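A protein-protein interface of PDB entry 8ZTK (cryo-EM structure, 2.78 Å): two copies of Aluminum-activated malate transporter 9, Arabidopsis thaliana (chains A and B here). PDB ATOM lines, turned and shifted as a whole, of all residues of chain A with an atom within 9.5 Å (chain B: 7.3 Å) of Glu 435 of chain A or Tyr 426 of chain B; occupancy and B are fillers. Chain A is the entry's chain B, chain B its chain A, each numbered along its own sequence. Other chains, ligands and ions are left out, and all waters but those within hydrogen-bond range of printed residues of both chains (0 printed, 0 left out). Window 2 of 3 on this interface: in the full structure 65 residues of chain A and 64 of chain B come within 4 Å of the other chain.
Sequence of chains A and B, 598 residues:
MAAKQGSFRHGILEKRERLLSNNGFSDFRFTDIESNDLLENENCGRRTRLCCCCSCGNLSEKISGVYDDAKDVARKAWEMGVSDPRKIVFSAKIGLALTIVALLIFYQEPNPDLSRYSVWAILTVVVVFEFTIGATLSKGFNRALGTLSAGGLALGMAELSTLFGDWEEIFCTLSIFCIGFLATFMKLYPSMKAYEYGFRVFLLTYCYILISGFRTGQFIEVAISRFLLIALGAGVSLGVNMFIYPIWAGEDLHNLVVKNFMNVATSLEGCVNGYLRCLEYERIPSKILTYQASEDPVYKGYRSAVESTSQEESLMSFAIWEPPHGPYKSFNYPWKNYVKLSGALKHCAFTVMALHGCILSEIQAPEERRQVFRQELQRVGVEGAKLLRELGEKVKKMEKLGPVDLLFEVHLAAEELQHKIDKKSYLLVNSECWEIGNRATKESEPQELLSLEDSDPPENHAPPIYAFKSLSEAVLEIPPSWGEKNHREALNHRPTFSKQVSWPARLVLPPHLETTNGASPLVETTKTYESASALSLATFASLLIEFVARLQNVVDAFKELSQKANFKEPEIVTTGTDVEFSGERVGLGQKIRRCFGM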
ATOM      1  N   SER A 425      14.268 -23.222  14.350  1.00  0.00           N
ATOM      2  CA  SER A 425      14.380 -22.152  13.368  1.00  0.00           C
ATOM      3  C   SER A 425      13.044 -21.750  12.760  1.00  0.00           C
ATOM      4  O   SER A 425      13.014 -20.848  11.917  1.00  0.00           O
ATOM      5  CB  SER A 425      15.345 -22.562  12.250  1.00  0.00           C
ATOM      6  OG  SER A 425      14.948 -23.784  11.654  1.00  0.00           O
ATOM      7  N   VAL A 429      11.055 -17.343  10.581  1.00  0.00           N
ATOM      8  CA  VAL A 429      10.511 -17.191   9.243  1.00  0.00           C
ATOM      9  C   VAL A 429       9.022 -17.523   9.279  1.00  0.00           C
ATOM     10  O   VAL A 429       8.471 -17.892  10.315  1.00  0.00           O
ATOM     11  CB  VAL A 429      11.246 -18.070   8.209  1.00  0.00           C
ATOM     12  CG1 VAL A 429      12.729 -17.733   8.185  1.00  0.00           C
ATOM     13  CG2 VAL A 429      11.029 -19.543   8.518  1.00  0.00           C
ATOM     14  N   ASN A 430       8.373 -17.378   8.125  1.00  0.00           N
ATOM     15  CA  ASN A 430       6.956 -17.689   7.959  1.00  0.00           C
ATOM     16  C   ASN A 430       6.819 -18.762   6.887  1.00  0.00           C
ATOM     17  O   ASN A 430       7.047 -18.494   5.702  1.00  0.00           O
ATOM     18  CB  ASN A 430       6.161 -16.439   7.589  1.00  0.00           C
ATOM     19  CG  ASN A 430       5.929 -15.524   8.774  1.00  0.00           C
ATOM     20  OD1 ASN A 430       6.714 -14.611   9.032  1.00  0.00           O
ATOM     21  ND2 ASN A 430       4.846 -15.766   9.505  1.00  0.00           N
ATOM     22  N   SER A 431       6.451 -19.975   7.301  1.00  0.00           N
ATOM     23  CA  SER A 431       6.348 -21.089   6.368  1.00  0.00           C
ATOM     24  C   SER A 431       5.071 -21.052   5.539  1.00  0.00           C
ATOM     25  O   SER A 431       5.019 -21.685   4.478  1.00  0.00           O
ATOM     26  CB  SER A 431       6.427 -22.417   7.124  1.00  0.00           C
ATOM     27  OG  SER A 431       5.632 -22.385   8.296  1.00  0.00           O
ATOM     28  N   GLU A 432       4.042 -20.332   5.993  1.00  0.00           N
ATOM     29  CA  GLU A 432       2.788 -20.285   5.248  1.00  0.00           C
ATOM     30  C   GLU A 432       2.987 -19.693   3.859  1.00  0.00           C
ATOM     31  O   GLU A 432       2.367 -20.145   2.890  1.00  0.00           O
ATOM     32  CB  GLU A 432       1.743 -19.485   6.026  1.00  0.00           C
ATOM     33  CG  GLU A 432       2.321 -18.382   6.895  1.00  0.00           C
ATOM     34  CD  GLU A 432       2.432 -18.787   8.351  1.00  0.00           C
ATOM     35  OE1 GLU A 432       3.056 -19.830   8.633  1.00  0.00           O
ATOM     36  OE2 GLU A 432       1.895 -18.061   9.213  1.00  0.00           O
ATOM     37  N   CYS A 433       3.846 -18.683   3.741  1.00  0.00           N
ATOM     38  CA  CYS A 433       4.051 -17.994   2.473  1.00  0.00           C
ATOM     39  C   CYS A 433       5.024 -18.712   1.547  1.00  0.00           C
ATOM     40  O   CYS A 433       5.221 -18.257   0.415  1.00  0.00           O
ATOM     41  CB  CYS A 433       4.546 -16.568   2.728  1.00  0.00           C
ATOM     42  SG  CYS A 433       3.356 -15.504   3.574  1.00  0.00           S
ATOM     43  N   TRP A 434       5.638 -19.805   1.994  1.00  0.00           N
ATOM     44  CA  TRP A 434       6.635 -20.490   1.181  1.00  0.00           C
ATOM     45  C   TRP A 434       6.055 -20.873  -0.175  1.00  0.00           C
ATOM     46  O   TRP A 434       4.965 -21.446  -0.260  1.00  0.00           O
ATOM     47  CB  TRP A 434       7.149 -21.732   1.906  1.00  0.00           C
ATOM     48  CG  TRP A 434       8.362 -21.470   2.740  1.00  0.00           C
ATOM     49  CD1 TRP A 434       9.125 -20.341   2.742  1.00  0.00           C
ATOM     50  CD2 TRP A 434       8.963 -22.363   3.684  1.00  0.00           C
ATOM     51  NE1 TRP A 434      10.158 -20.469   3.636  1.00  0.00           N
ATOM     52  CE2 TRP A 434      10.084 -21.703   4.227  1.00  0.00           C
ATOM     53  CE3 TRP A 434       8.662 -23.655   4.126  1.00  0.00           C
ATOM     54  CZ2 TRP A 434      10.902 -22.290   5.187  1.00  0.00           C
ATOM     55  CZ3 TRP A 434       9.477 -24.235   5.080  1.00  0.00           C
ATOM     56  CH2 TRP A 434      10.583 -23.553   5.600  1.00  0.00           C
ATOM     57  N   GLU A 435       6.790 -20.553  -1.236  1.00  0.00           N
ATOM     58  CA  GLU A 435       6.356 -20.870  -2.592  1.00  0.00           C
ATOM     59  C   GLU A 435       7.488 -21.504  -3.393  1.00  0.00           C
ATOM     60  O   GLU A 435       8.500 -20.862  -3.671  1.00  0.00           O
ATOM     61  CB  GLU A 435       5.848 -19.614  -3.302  1.00  0.00           C
ATOM     62  CG  GLU A 435       6.844 -18.468  -3.328  1.00  0.00           C
ATOM     63  CD  GLU A 435       6.651 -17.554  -4.521  1.00  0.00           C
ATOM     64  OE1 GLU A 435       5.622 -16.850  -4.571  1.00  0.00           O
ATOM     65  OE2 GLU A 435       7.529 -17.542  -5.410  1.00  0.00           O
ATOM     66  N   LEU A 535      12.934 -11.789  12.085  1.00  0.00           N
ATOM     67  CA  LEU A 535      14.246 -11.931  11.464  1.00  0.00           C
ATOM     68  C   LEU A 535      15.349 -11.168  12.191  1.00  0.00           C
ATOM     69  O   LEU A 535      16.520 -11.315  11.828  1.00  0.00           O
ATOM     70  CB  LEU A 535      14.185 -11.472  10.005  1.00  0.00           C
ATOM     71  CG  LEU A 535      15.150 -12.152   9.031  1.00  0.00           C
ATOM     72  CD1 LEU A 535      14.647 -13.536   8.653  1.00  0.00           C
ATOM     73  CD2 LEU A 535      15.352 -11.297   7.791  1.00  0.00           C
ATOM     74  N   ARG B 369      23.240 -18.401  -4.228  1.00  0.00           N
ATOM     75  CA  ARG B 369      22.056 -18.039  -3.459  1.00  0.00           C
ATOM     76  C   ARG B 369      21.882 -16.535  -3.297  1.00  0.00           C
ATOM     77  O   ARG B 369      20.773 -16.085  -2.985  1.00  0.00           O
ATOM     78  CB  ARG B 369      22.094 -18.705  -2.081  1.00  0.00           C
ATOM     79  CG  ARG B 369      22.071 -20.221  -2.143  1.00  0.00           C
ATOM     80  CD  ARG B 369      21.450 -20.827  -0.898  1.00  0.00           C
ATOM     81  NE  ARG B 369      22.167 -22.018  -0.462  1.00  0.00           N
ATOM     82  CZ  ARG B 369      21.779 -22.809   0.528  1.00  0.00           C
ATOM     83  NH1 ARG B 369      20.677 -22.562   1.218  1.00  0.00           N
ATOM     84  NH2 ARG B 369      22.515 -23.873   0.836  1.00  0.00           N
ATOM     85  N   HIS B 419       8.568  -8.627   1.104  1.00  0.00           N
ATOM     86  CA  HIS B 419       7.715  -9.626   0.462  1.00  0.00           C
ATOM     87  C   HIS B 419       8.542 -10.698  -0.238  1.00  0.00           C
ATOM     88  O   HIS B 419       8.250 -11.897  -0.125  1.00  0.00           O
ATOM     89  CB  HIS B 419       6.765  -8.955  -0.530  1.00  0.00           C
ATOM     90  CG  HIS B 419       5.663  -8.176   0.119  1.00  0.00           C
ATOM     91  ND1 HIS B 419       4.872  -7.288  -0.578  1.00  0.00           N
ATOM     92  CD2 HIS B 419       5.217  -8.157   1.396  1.00  0.00           C
ATOM     93  CE1 HIS B 419       3.987  -6.753   0.245  1.00  0.00           C
ATOM     94  NE2 HIS B 419       4.175  -7.262   1.448  1.00  0.00           N
ATOM     95  N   LYS B 420       9.590 -10.287  -0.957  1.00  0.00           N
ATOM     96  CA  LYS B 420      10.428 -11.264  -1.645  1.00  0.00           C
ATOM     97  C   LYS B 420      11.107 -12.196  -0.653  1.00  0.00           C
ATOM     98  O   LYS B 420      11.198 -13.407  -0.890  1.00  0.00           O
ATOM     99  CB  LYS B 420      11.465 -10.552  -2.513  1.00  0.00           C
ATOM    100  CG  LYS B 420      12.374 -11.496  -3.277  1.00  0.00           C
ATOM    101  CD  LYS B 420      11.582 -12.359  -4.245  1.00  0.00           C
ATOM    102  CE  LYS B 420      12.472 -12.921  -5.340  1.00  0.00           C
ATOM    103  NZ  LYS B 420      11.866 -12.750  -6.688  1.00  0.00           N
ATOM    104  N   ILE B 421      11.594 -11.655   0.465  1.00  0.00           N
ATOM    105  CA  ILE B 421      12.256 -12.501   1.453  1.00  0.00           C
ATOM    106  C   ILE B 421      11.262 -13.496   2.036  1.00  0.00           C
ATOM    107  O   ILE B 421      11.593 -14.666   2.269  1.00  0.00           O
ATOM    108  CB  ILE B 421      12.914 -11.647   2.553  1.00  0.00           C
ATOM    109  CG1 ILE B 421      13.972 -10.721   1.955  1.00  0.00           C
ATOM    110  CG2 ILE B 421      13.531 -12.535   3.620  1.00  0.00           C
ATOM    111  CD1 ILE B 421      14.499  -9.694   2.932  1.00  0.00           C
ATOM    112  N   ASP B 422      10.028 -13.049   2.278  1.00  0.00           N
ATOM    113  CA  ASP B 422       9.009 -13.946   2.815  1.00  0.00           C
ATOM    114  C   ASP B 422       8.662 -15.055   1.829  1.00  0.00           C
ATOM    115  O   ASP B 422       8.383 -16.189   2.236  1.00  0.00           O
ATOM    116  CB  ASP B 422       7.758 -13.153   3.189  1.00  0.00           C
ATOM    117  CG  ASP B 422       7.729 -12.768   4.653  1.00  0.00           C
ATOM    118  OD1 ASP B 422       8.766 -12.929   5.330  1.00  0.00           O
ATOM    119  OD2 ASP B 422       6.671 -12.303   5.126  1.00  0.00           O
ATOM    120  N   LYS B 423       8.674 -14.753   0.528  1.00  0.00           N
ATOM    121  CA  LYS B 423       8.345 -15.775  -0.465  1.00  0.00           C
ATOM    122  C   LYS B 423       9.412 -16.864  -0.547  1.00  0.00           C
ATOM    123  O   LYS B 423       9.087 -18.036  -0.767  1.00  0.00           O
ATOM    124  CB  LYS B 423       8.138 -15.130  -1.835  1.00  0.00           C
ATOM    125  CG  LYS B 423       6.679 -14.972  -2.233  1.00  0.00           C
ATOM    126  CD  LYS B 423       5.849 -14.369  -1.112  1.00  0.00           C
ATOM    127  CE  LYS B 423       5.652 -12.875  -1.310  1.00  0.00           C
ATOM    128  NZ  LYS B 423       4.935 -12.255  -0.161  1.00  0.00           N
ATOM    129  N   LYS B 424      10.684 -16.507  -0.374  1.00  0.00           N
ATOM    130  CA  LYS B 424      11.768 -17.474  -0.525  1.00  0.00           C
ATOM    131  C   LYS B 424      12.643 -17.574   0.719  1.00  0.00           C
ATOM    132  O   LYS B 424      13.860 -17.375   0.642  1.00  0.00           O
ATOM    133  CB  LYS B 424      12.629 -17.119  -1.739  1.00  0.00           C
ATOM    134  CG  LYS B 424      12.215 -17.830  -3.014  1.00  0.00           C
ATOM    135  CD  LYS B 424      12.177 -16.880  -4.196  1.00  0.00           C
ATOM    136  CE  LYS B 424      11.171 -17.342  -5.236  1.00  0.00           C
ATOM    137  NZ  LYS B 424      11.435 -18.740  -5.676  1.00  0.00           N
ATOM    138  N   SER B 425      12.043 -17.888   1.864  1.00  0.00           N
ATOM    139  CA  SER B 425      12.777 -17.964   3.120  1.00  0.00           C
ATOM    140  C   SER B 425      13.260 -19.370   3.453  1.00  0.00           C
ATOM    141  O   SER B 425      13.898 -19.555   4.493  1.00  0.00           O
ATOM    142  CB  SER B 425      11.910 -17.439   4.270  1.00  0.00           C
ATOM    143  OG  SER B 425      10.677 -18.133   4.338  1.00  0.00           O
ATOM    144  N   TYR B 426      12.980 -20.360   2.606  1.00  0.00           N
ATOM    145  CA  TYR B 426      13.447 -21.717   2.863  1.00  0.00           C
ATOM    146  C   TYR B 426      14.910 -21.911   2.490  1.00  0.00           C
ATOM    147  O   TYR B 426      15.438 -23.015   2.662  1.00  0.00           O
ATOM    148  CB  TYR B 426      12.577 -22.733   2.114  1.00  0.00           C
ATOM    149  CG  TYR B 426      12.524 -22.543   0.615  1.00  0.00           C
ATOM    150  CD1 TYR B 426      13.600 -22.896  -0.189  1.00  0.00           C
ATOM    151  CD2 TYR B 426      11.389 -22.036   0.001  1.00  0.00           C
ATOM    152  CE1 TYR B 426      13.554 -22.732  -1.557  1.00  0.00           C
ATOM    153  CE2 TYR B 426      11.334 -21.867  -1.368  1.00  0.00           C
ATOM    154  CZ  TYR B 426      12.419 -22.218  -2.142  1.00  0.00           C
ATOM    155  OH  TYR B 426      12.371 -22.054  -3.506  1.00  0.00           O
ATOM    156  N   LEU B 427      15.569 -20.873   1.983  1.00  0.00           N
ATOM    157  CA  LEU B 427      16.972 -20.927   1.597  1.00  0.00           C
ATOM    158  C   LEU B 427      17.907 -20.479   2.710  1.00  0.00           C
ATOM    159  O   LEU B 427      19.128 -20.502   2.524  1.00  0.00           O
ATOM    160  CB  LEU B 427      17.211 -20.063   0.353  1.00  0.00           C
ATOM    161  CG  LEU B 427      16.391 -20.396  -0.892  1.00  0.00           C
ATOM    162  CD1 LEU B 427      16.657 -19.379  -1.991  1.00  0.00           C
ATOM    163  CD2 LEU B 427      16.707 -21.802  -1.374  1.00  0.00           C
ATOM    164  N   LEU B 428      17.366 -20.071   3.860  1.00  0.00           N
ATOM    165  CA  LEU B 428      18.173 -19.575   4.964  1.00  0.00           C
ATOM    166  C   LEU B 428      18.194 -20.500   6.171  1.00  0.00           C
ATOM    167  O   LEU B 428      19.091 -20.368   7.010  1.00  0.00           O
ATOM    168  CB  LEU B 428      17.669 -18.193   5.410  1.00  0.00           C
ATOM    169  CG  LEU B 428      17.325 -17.202   4.295  1.00  0.00           C
ATOM    170  CD1 LEU B 428      16.479 -16.061   4.835  1.00  0.00           C
ATOM    171  CD2 LEU B 428      18.583 -16.673   3.627  1.00  0.00           C
ATOM    172  N   VAL B 429      17.246 -21.427   6.278  1.00  0.00           N
ATOM    173  CA  VAL B 429      17.147 -22.335   7.408  1.00  0.00           C
ATOM    174  C   VAL B 429      17.134 -23.769   6.885  1.00  0.00           C
ATOM    175  O   VAL B 429      17.162 -24.014   5.680  1.00  0.00           O
ATOM    176  CB  VAL B 429      15.904 -22.054   8.277  1.00  0.00           C
ATOM    177  CG1 VAL B 429      15.928 -20.622   8.790  1.00  0.00           C
ATOM    178  CG2 VAL B 429      14.633 -22.328   7.487  1.00  0.00           C
ATOM    179  N   ASN B 430      17.096 -24.719   7.817  1.00  0.00           N
ATOM    180  CA  ASN B 430      17.036 -26.145   7.505  1.00  0.00           C
ATOM    181  C   ASN B 430      15.769 -26.720   8.123  1.00  0.00           C
ATOM    182  O   ASN B 430      15.670 -26.839   9.349  1.00  0.00           O
ATOM    183  CB  ASN B 430      18.278 -26.871   8.020  1.00  0.00           C
ATOM    184  CG  ASN B 430      19.496 -26.627   7.152  1.00  0.00           C
ATOM    185  OD1 ASN B 430      20.273 -25.705   7.400  1.00  0.00           O
ATOM    186  ND2 ASN B 430      19.670 -27.453   6.128  1.00  0.00           N
ATOM    187  N   SER B 431      14.802 -27.077   7.276  1.00  0.00           N
ATOM    188  CA  SER B 431      13.526 -27.584   7.763  1.00  0.00           C
ATOM    189  C   SER B 431      13.594 -29.040   8.202  1.00  0.00           C
ATOM    190  O   SER B 431      12.729 -29.484   8.965  1.00  0.00           O
ATOM    191  CB  SER B 431      12.451 -27.423   6.686  1.00  0.00           C
ATOM    192  OG  SER B 431      12.942 -27.814   5.415  1.00  0.00           O
ATOM    193  N   TRP B 434      13.738 -29.450  11.976  1.00  0.00           N
ATOM    194  CA  TRP B 434      12.685 -28.833  12.771  1.00  0.00           C
ATOM    195  C   TRP B 434      12.083 -29.838  13.745  1.00  0.00           C
ATOM    196  O   TRP B 434      11.731 -30.958  13.363  1.00  0.00           O
ATOM    197  CB  TRP B 434      11.598 -28.262  11.861  1.00  0.00           C
ATOM    198  CG  TRP B 434      11.827 -26.832  11.493  1.00  0.00           C
ATOM    199  CD1 TRP B 434      12.747 -25.984  12.036  1.00  0.00           C
ATOM    200  CD2 TRP B 434      11.112 -26.072  10.512  1.00  0.00           C
ATOM    201  NE1 TRP B 434      12.656 -24.747  11.447  1.00  0.00           N
ATOM    202  CE2 TRP B 434      11.659 -24.774  10.509  1.00  0.00           C
ATOM    203  CE3 TRP B 434      10.064 -26.364   9.634  1.00  0.00           C
ATOM    204  CZ2 TRP B 434      11.195 -23.771   9.662  1.00  0.00           C
ATOM    205  CZ3 TRP B 434       9.604 -25.367   8.795  1.00  0.00           C
ATOM    206  CH2 TRP B 434      10.170 -24.087   8.815  1.00  0.00           C
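The backbone carbonyl oxygen (O) of Lys 423 of chain B sits close to the backbone NH (N) of Glu 435 of chain A (3.4 Å). The indole nitrogen (NE1) of Trp 434 of chain B is in hydrogen-bond range of the side-chain hydroxyl (OG) of Ser 425 of chain A, at 2.5 Å. The indole nitrogen of Trp 434 of chain A lies within hydrogen-bond range of the side-chain hydroxyl of Ser 425 of chain B, at 2.5 Å. The backbone NH (N) of Tyr 426 of chain B lies close to the indole nitrogen (NE1) of Trp 434 of chain A, at 3.0 Å.
The backbone carbonyl oxygen of His 419 of chain B lies close to the side-chain amino group of Lys 423 of chain B (3.3 Å).
OG of Ser 425 of chain A touches CB of Val 429 of chain B (3.9 Å). Ser 425 of chain A touches Asn 430 of chain B (OG to O, 3.9 Å). CB of Val 429 of chain A touches OG of Ser 425 of chain B, 3.9 Å away. Ser 425 of chain B touches Asn 430 of chain A (OG to O, 3.9 Å). Asp 422 of chain B touches Cys 433 of chain A. Lys 423 of chain B touches Trp 434 of chain A. Trp 434 of chain A touches Trp 434 of chain B. Glu 435 of chain A touches Lys 424 of chain B (OE2 to CE, 3.7 Å). Tyr 426 of chain B touches Glu 435 of chain A (CE2 to O, 3.8 Å).
Of chain A, only Trp 434 and Glu 435 come within 4 Å of Tyr 426 of chain B. Lys 424 of chain B touches just one residue of chain A: Glu 435. Of chain A, only Val 429, Asn 430 and Trp 434 come within 4 Å of Ser 425 of chain B. Leu 427 of chain B touches none of the printed residues of chain A. Printed residues of chain B within 4 Å of Val 429 of chain A: Ser 425. Printed residues of chain A within 4 Å of Asp 422 of chain B: Cys 433 (3.9 Å). Of the printed residues of chain A, Val 429 of chain B touches Ser 425. Printed residues of chain B within 4 Å of Trp 434 of chain A: Lys 423, Ser 425, Tyr 426 and Trp 434. Leu 428 of chain B touches none of the printed residues of chain A. Ser 431 of chain B touches none of the printed residues of chain A. The nearest residue of chain A that does not touch Tyr 426 of chain B is Val 429 of chain A (6.2 Å).
Of the 15 printed residues of chain B, 8 touch a printed residue of chain A. Of the 9 printed residues of chain A, 6 touch a printed residue of chain B. Hydrophobic or aromatic side chains of chain A that line the printed part of chain B: Val 429 and Trp 434. Among the printed residues, no Asp or Glu carboxylate lies within 4 Å of a Lys or Arg side-chain nitrogen of the other chain.
Ser 425 of chain A touches Val 429 of chain B, and with the chains exchanged Val 429 of chain A touches Ser 425 of chain B. Ser 425 of chain A touches Asn 430 of chain B, and with the chains exchanged Asn 430 of chain A touches Ser 425 of chain B. Ser 425 of chain A touches Trp 434 of chain B, and with the chains exchanged Trp 434 of chain A touches Ser 425 of chain B. Trp 434 of chain B touches its own counterpart, Trp 434 of chain A. Of the 13 pairs that touch across the chains among the printed residues, 7 have their exchanged pair printed and touching as well.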
